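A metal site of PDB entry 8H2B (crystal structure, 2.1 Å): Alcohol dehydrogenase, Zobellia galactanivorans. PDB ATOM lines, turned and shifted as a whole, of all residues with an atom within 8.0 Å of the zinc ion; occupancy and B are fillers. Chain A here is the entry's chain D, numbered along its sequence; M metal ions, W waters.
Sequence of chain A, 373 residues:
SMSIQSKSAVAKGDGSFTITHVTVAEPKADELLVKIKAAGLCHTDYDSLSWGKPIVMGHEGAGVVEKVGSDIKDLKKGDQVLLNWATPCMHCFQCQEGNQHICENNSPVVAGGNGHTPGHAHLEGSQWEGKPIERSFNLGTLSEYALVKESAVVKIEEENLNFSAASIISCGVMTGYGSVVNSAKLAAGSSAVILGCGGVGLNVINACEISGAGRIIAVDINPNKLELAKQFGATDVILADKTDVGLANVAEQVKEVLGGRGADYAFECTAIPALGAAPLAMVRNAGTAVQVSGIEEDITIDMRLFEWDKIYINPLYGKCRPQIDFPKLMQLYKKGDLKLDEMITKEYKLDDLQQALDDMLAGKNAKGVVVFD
The side-chain carboxylate (OE1) of Glu 60 is in salt-bridge range of the side-chain amino group (NZ) of Lys 367 (2.9 Å). N of Gly 40 is in hydrogen-bond range of O of Glu 60 (3.4 Å). The side-chain sulfur of Cys 42 lies close to the backbone NH of Thr 44, at 3.5 Å. OD1 of Asp 45 is in hydrogen-bond range of ND1 of His 59 (2.7 Å). OG1 of Thr 175 is in hydrogen-bond range of O of Cys 171 (2.7 Å). The backbone NH of Cys 42 lies within hydrogen-bond range of the side-chain carboxylate of Asp 45, at 3.2 Å.
Four residues have an atom within 4 Å of the zinc ion: Cys 42, His 59, Glu 60 and Cys 171.
OE2 of Glu 60 binds the zinc ion (2.2 Å). The zinc ion is bound by a ring nitrogen (NE2) of His 59, at 2.3 Å. The zinc ion is bound by the side-chain sulfur (SG) of Cys 42, at 2.3 Å. SG of Cys 171 is bound to the zinc ion, 2.4 Å away. The zinc ion has four donor atoms within binding distance.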
ATOM      1  N   GLY A  40      21.833 -23.816 -20.754  1.00  0.00           N
ATOM      2  CA  GLY A  40      22.334 -22.719 -19.948  1.00  0.00           C
ATOM      3  C   GLY A  40      23.536 -23.125 -19.114  1.00  0.00           C
ATOM      4  O   GLY A  40      23.778 -24.293 -18.824  1.00  0.00           O
ATOM      5  N   LEU A  41      24.317 -22.123 -18.725  1.00  0.00           N
ATOM      6  CA  LEU A  41      25.523 -22.330 -17.946  1.00  0.00           C
ATOM      7  C   LEU A  41      25.422 -21.568 -16.637  1.00  0.00           C
ATOM      8  O   LEU A  41      24.975 -20.423 -16.636  1.00  0.00           O
ATOM      9  CB  LEU A  41      26.755 -21.818 -18.695  1.00  0.00           C
ATOM     10  CG  LEU A  41      27.224 -22.536 -19.950  1.00  0.00           C
ATOM     11  CD1 LEU A  41      26.289 -22.227 -21.088  1.00  0.00           C
ATOM     12  CD2 LEU A  41      28.628 -22.022 -20.259  1.00  0.00           C
ATOM     13  N   CYS A  42      25.843 -22.196 -15.538  1.00  0.00           N
ATOM     14  CA  CYS A  42      26.002 -21.451 -14.284  1.00  0.00           C
ATOM     15  C   CYS A  42      27.187 -22.029 -13.519  1.00  0.00           C
ATOM     16  O   CYS A  42      27.865 -22.951 -13.975  1.00  0.00           O
ATOM     17  CB  CYS A  42      24.733 -21.479 -13.407  1.00  0.00           C
ATOM     18  SG  CYS A  42      24.416 -23.010 -12.519  1.00  0.00           S
ATOM     19  N   HIS A  43      27.424 -21.468 -12.332  1.00  0.00           N
ATOM     20  CA  HIS A  43      28.613 -21.817 -11.559  1.00  0.00           C
ATOM     21  C   HIS A  43      28.668 -23.293 -11.197  1.00  0.00           C
ATOM     22  O   HIS A  43      29.755 -23.848 -11.016  1.00  0.00           O
ATOM     23  CB  HIS A  43      28.668 -20.973 -10.288  1.00  0.00           C
ATOM     24  CG  HIS A  43      30.046 -20.867  -9.724  1.00  0.00           C
ATOM     25  ND1 HIS A  43      30.659 -21.913  -9.051  1.00  0.00           N
ATOM     26  CD2 HIS A  43      30.959 -19.865  -9.760  1.00  0.00           C
ATOM     27  CE1 HIS A  43      31.880 -21.539  -8.684  1.00  0.00           C
ATOM     28  NE2 HIS A  43      32.076 -20.306  -9.100  1.00  0.00           N
ATOM     29  N   THR A  44      27.517 -23.959 -11.089  1.00  0.00           N
ATOM     30  CA  THR A  44      27.522 -25.371 -10.727  1.00  0.00           C
ATOM     31  C   THR A  44      28.257 -26.202 -11.752  1.00  0.00           C
ATOM     32  O   THR A  44      28.917 -27.202 -11.401  1.00  0.00           O
ATOM     33  CB  THR A  44      26.084 -25.867 -10.565  1.00  0.00           C
ATOM     34  OG1 THR A  44      25.474 -25.207  -9.439  1.00  0.00           O
ATOM     35  CG2 THR A  44      26.047 -27.373 -10.346  1.00  0.00           C
ATOM     36  N   ASP A  45      28.189 -25.819 -13.024  1.00  0.00           N
ATOM     37  CA  ASP A  45      28.894 -26.561 -14.057  1.00  0.00           C
ATOM     38  C   ASP A  45      30.408 -26.432 -13.899  1.00  0.00           C
ATOM     39  O   ASP A  45      31.135 -27.406 -14.129  1.00  0.00           O
ATOM     40  CB  ASP A  45      28.425 -26.086 -15.430  1.00  0.00           C
ATOM     41  CG  ASP A  45      26.933 -26.254 -15.611  1.00  0.00           C
ATOM     42  OD1 ASP A  45      26.425 -27.365 -15.298  1.00  0.00           O
ATOM     43  OD2 ASP A  45      26.262 -25.298 -16.065  1.00  0.00           O
ATOM     44  N   GLY A  58      26.375 -30.182 -17.648  1.00  0.00           N
ATOM     45  CA  GLY A  58      25.154 -29.485 -17.999  1.00  0.00           C
ATOM     46  C   GLY A  58      23.932 -29.967 -17.240  1.00  0.00           C
ATOM     47  O   GLY A  58      23.626 -31.160 -17.238  1.00  0.00           O
ATOM     48  N   HIS A  59      23.220 -29.019 -16.595  1.00  0.00           N
ATOM     49  CA  HIS A  59      21.999 -29.317 -15.853  1.00  0.00           C
ATOM     50  C   HIS A  59      20.859 -28.358 -16.194  1.00  0.00           C
ATOM     51  O   HIS A  59      19.862 -28.329 -15.482  1.00  0.00           O
ATOM     52  CB  HIS A  59      22.303 -29.288 -14.352  1.00  0.00           C
ATOM     53  CG  HIS A  59      22.758 -27.949 -13.884  1.00  0.00           C
ATOM     54  ND1 HIS A  59      23.908 -27.357 -14.357  1.00  0.00           N
ATOM     55  CD2 HIS A  59      22.210 -27.080 -13.009  1.00  0.00           C
ATOM     56  CE1 HIS A  59      24.049 -26.178 -13.792  1.00  0.00           C
ATOM     57  NE2 HIS A  59      23.044 -25.995 -12.961  1.00  0.00           N
ATOM     58  N   GLU A  60      20.997 -27.590 -17.271  1.00  0.00           N
ATOM     59  CA  GLU A  60      19.969 -26.678 -17.760  1.00  0.00           C
ATOM     60  C   GLU A  60      19.833 -26.923 -19.253  1.00  0.00           C
ATOM     61  O   GLU A  60      20.845 -26.985 -19.958  1.00  0.00           O
ATOM     62  CB  GLU A  60      20.372 -25.209 -17.553  1.00  0.00           C
ATOM     63  CG  GLU A  60      20.962 -24.864 -16.199  1.00  0.00           C
ATOM     64  CD  GLU A  60      21.380 -23.396 -16.127  1.00  0.00           C
ATOM     65  OE1 GLU A  60      20.993 -22.626 -17.042  1.00  0.00           O
ATOM     66  OE2 GLU A  60      22.083 -23.010 -15.162  1.00  0.00           O
ATOM     67  N   TRP A  85      15.900 -30.676 -13.173  1.00  0.00           N
ATOM     68  CA  TRP A  85      16.739 -31.600 -12.434  1.00  0.00           C
ATOM     69  C   TRP A  85      16.073 -32.121 -11.171  1.00  0.00           C
ATOM     70  O   TRP A  85      16.732 -32.787 -10.374  1.00  0.00           O
ATOM     71  CB  TRP A  85      18.099 -30.988 -12.135  1.00  0.00           C
ATOM     72  CG  TRP A  85      18.128 -29.590 -11.533  1.00  0.00           C
ATOM     73  CD1 TRP A  85      18.282 -28.417 -12.212  1.00  0.00           C
ATOM     74  CD2 TRP A  85      18.105 -29.240 -10.142  1.00  0.00           C
ATOM     75  NE1 TRP A  85      18.305 -27.364 -11.345  1.00  0.00           N
ATOM     76  CE2 TRP A  85      18.210 -27.832 -10.063  1.00  0.00           C
ATOM     77  CE3 TRP A  85      17.986 -29.975  -8.955  1.00  0.00           C
ATOM     78  CZ2 TRP A  85      18.209 -27.148  -8.851  1.00  0.00           C
ATOM     79  CZ3 TRP A  85      17.986 -29.296  -7.766  1.00  0.00           C
ATOM     80  CH2 TRP A  85      18.095 -27.903  -7.715  1.00  0.00           C
ATOM     81  N   PHE A 137      23.421 -33.868 -12.583  1.00  0.00           N
ATOM     82  CA  PHE A 137      22.064 -33.617 -12.081  1.00  0.00           C
ATOM     83  C   PHE A 137      21.008 -34.464 -12.791  1.00  0.00           C
ATOM     84  O   PHE A 137      19.862 -34.037 -12.946  1.00  0.00           O
ATOM     85  CB  PHE A 137      21.704 -32.120 -12.153  1.00  0.00           C
ATOM     86  CG  PHE A 137      22.270 -31.323 -11.015  1.00  0.00           C
ATOM     87  CD1 PHE A 137      23.641 -31.095 -10.912  1.00  0.00           C
ATOM     88  CD2 PHE A 137      21.429 -30.786 -10.042  1.00  0.00           C
ATOM     89  CE1 PHE A 137      24.161 -30.360  -9.846  1.00  0.00           C
ATOM     90  CE2 PHE A 137      21.949 -30.051  -8.975  1.00  0.00           C
ATOM     91  CZ  PHE A 137      23.323 -29.835  -8.879  1.00  0.00           C
ATOM     92  N   SER A 167      15.966 -22.414 -22.390  1.00  0.00           N
ATOM     93  CA  SER A 167      16.936 -23.266 -21.726  1.00  0.00           C
ATOM     94  C   SER A 167      17.282 -22.775 -20.333  1.00  0.00           C
ATOM     95  O   SER A 167      17.835 -23.551 -19.545  1.00  0.00           O
ATOM     96  CB  SER A 167      18.219 -23.359 -22.559  1.00  0.00           C
ATOM     97  OG  SER A 167      18.902 -22.118 -22.611  1.00  0.00           O
ATOM     98  N   ILE A 168      16.984 -21.522 -19.983  1.00  0.00           N
ATOM     99  CA  ILE A 168      17.381 -21.041 -18.653  1.00  0.00           C
ATOM    100  C   ILE A 168      16.275 -21.170 -17.624  1.00  0.00           C
ATOM    101  O   ILE A 168      16.523 -20.933 -16.434  1.00  0.00           O
ATOM    102  CB  ILE A 168      17.889 -19.595 -18.725  1.00  0.00           C
ATOM    103  CG1 ILE A 168      16.788 -18.646 -19.220  1.00  0.00           C
ATOM    104  CG2 ILE A 168      19.138 -19.517 -19.652  1.00  0.00           C
ATOM    105  CD1 ILE A 168      17.156 -17.168 -19.086  1.00  0.00           C
ATOM    106  N   SER A 170      15.325 -23.836 -16.589  1.00  0.00           N
ATOM    107  CA  SER A 170      15.687 -25.083 -15.926  1.00  0.00           C
ATOM    108  C   SER A 170      16.282 -24.902 -14.545  1.00  0.00           C
ATOM    109  O   SER A 170      16.199 -25.835 -13.736  1.00  0.00           O
ATOM    110  CB  SER A 170      16.723 -25.835 -16.767  1.00  0.00           C
ATOM    111  OG  SER A 170      16.156 -26.492 -17.873  1.00  0.00           O
ATOM    112  N   CYS A 171      16.955 -23.789 -14.277  1.00  0.00           N
ATOM    113  CA  CYS A 171      17.731 -23.660 -13.037  1.00  0.00           C
ATOM    114  C   CYS A 171      17.553 -22.281 -12.398  1.00  0.00           C
ATOM    115  O   CYS A 171      16.797 -22.148 -11.425  1.00  0.00           O
ATOM    116  CB  CYS A 171      19.221 -23.927 -13.285  1.00  0.00           C
ATOM    117  SG  CYS A 171      20.368 -23.784 -11.836  1.00  0.00           S
ATOM    118  N   GLY A 172      18.238 -21.275 -12.934  1.00  0.00           N
ATOM    119  CA  GLY A 172      18.258 -19.964 -12.301  1.00  0.00           C
ATOM    120  C   GLY A 172      16.906 -19.276 -12.283  1.00  0.00           C
ATOM    121  O   GLY A 172      16.544 -18.634 -11.302  1.00  0.00           O
ATOM    122  N   VAL A 173      16.158 -19.390 -13.378  1.00  0.00           N
ATOM    123  CA  VAL A 173      14.837 -18.773 -13.441  1.00  0.00           C
ATOM    124  C   VAL A 173      13.889 -19.431 -12.441  1.00  0.00           C
ATOM    125  O   VAL A 173      13.261 -18.758 -11.619  1.00  0.00           O
ATOM    126  CB  VAL A 173      14.285 -18.849 -14.886  1.00  0.00           C
ATOM    127  CG1 VAL A 173      12.807 -18.410 -14.933  1.00  0.00           C
ATOM    128  CG2 VAL A 173      15.139 -18.005 -15.828  1.00  0.00           C
ATOM    129  N   THR A 175      14.636 -21.093  -9.836  1.00  0.00           N
ATOM    130  CA  THR A 175      15.097 -20.902  -8.467  1.00  0.00           C
ATOM    131  C   THR A 175      14.723 -19.514  -7.949  1.00  0.00           C
ATOM    132  O   THR A 175      14.145 -19.375  -6.859  1.00  0.00           O
ATOM    133  CB  THR A 175      16.604 -21.138  -8.400  1.00  0.00           C
ATOM    134  OG1 THR A 175      16.887 -22.496  -8.789  1.00  0.00           O
ATOM    135  CG2 THR A 175      17.139 -20.906  -6.987  1.00  0.00           C
ATOM    136  N   VAL A 200      20.586 -15.842 -10.524  1.00  0.00           N
ATOM    137  CA  VAL A 200      19.465 -16.054  -9.600  1.00  0.00           C
ATOM    138  C   VAL A 200      18.849 -14.719  -9.203  1.00  0.00           C
ATOM    139  O   VAL A 200      17.643 -14.521  -9.316  1.00  0.00           O
ATOM    140  CB  VAL A 200      19.922 -16.870  -8.377  1.00  0.00           C
ATOM    141  CG1 VAL A 200      18.772 -17.050  -7.421  1.00  0.00           C
ATOM    142  CG2 VAL A 200      20.476 -18.238  -8.816  1.00  0.00           C
ATOM    143  N   TYR A 317      15.592 -24.956  -5.156  1.00  0.00           N
ATOM    144  CA  TYR A 317      15.077 -24.979  -6.533  1.00  0.00           C
ATOM    145  C   TYR A 317      13.722 -24.296  -6.624  1.00  0.00           C
ATOM    146  O   TYR A 317      12.860 -24.652  -7.430  1.00  0.00           O
ATOM    147  CB  TYR A 317      15.062 -26.429  -7.040  1.00  0.00           C
ATOM    148  CG  TYR A 317      14.840 -26.702  -8.517  1.00  0.00           C
ATOM    149  CD1 TYR A 317      15.368 -25.856  -9.477  1.00  0.00           C
ATOM    150  CD2 TYR A 317      14.440 -27.977  -8.946  1.00  0.00           C
ATOM    151  CE1 TYR A 317      15.277 -26.145 -10.846  1.00  0.00           C
ATOM    152  CE2 TYR A 317      14.369 -28.302 -10.317  1.00  0.00           C
ATOM    153  CZ  TYR A 317      14.802 -27.378 -11.260  1.00  0.00           C
ATOM    154  OH  TYR A 317      14.744 -27.650 -12.602  1.00  0.00           O
ATOM    155  N   LYS A 367      23.417 -14.383 -18.213  1.00  0.00           N
ATOM    156  CA  LYS A 367      23.472 -15.816 -18.489  1.00  0.00           C
ATOM    157  C   LYS A 367      24.164 -16.028 -19.827  1.00  0.00           C
ATOM    158  O   LYS A 367      23.925 -15.287 -20.775  1.00  0.00           O
ATOM    159  CB  LYS A 367      22.071 -16.445 -18.543  1.00  0.00           C
ATOM    160  CG  LYS A 367      21.356 -16.539 -17.203  1.00  0.00           C
ATOM    161  CD  LYS A 367      21.956 -17.626 -16.333  1.00  0.00           C
ATOM    162  CE  LYS A 367      21.757 -19.006 -16.947  1.00  0.00           C
ATOM    163  NZ  LYS A 367      22.017 -20.088 -15.960  1.00  0.00           N
HETATM  164 ZN    ZN M   1      22.334 -23.844 -13.180  1.00  0.00          ZN
HETATM  165  O   HOH W   1      22.224 -24.908 -10.507  1.00  0.00           O
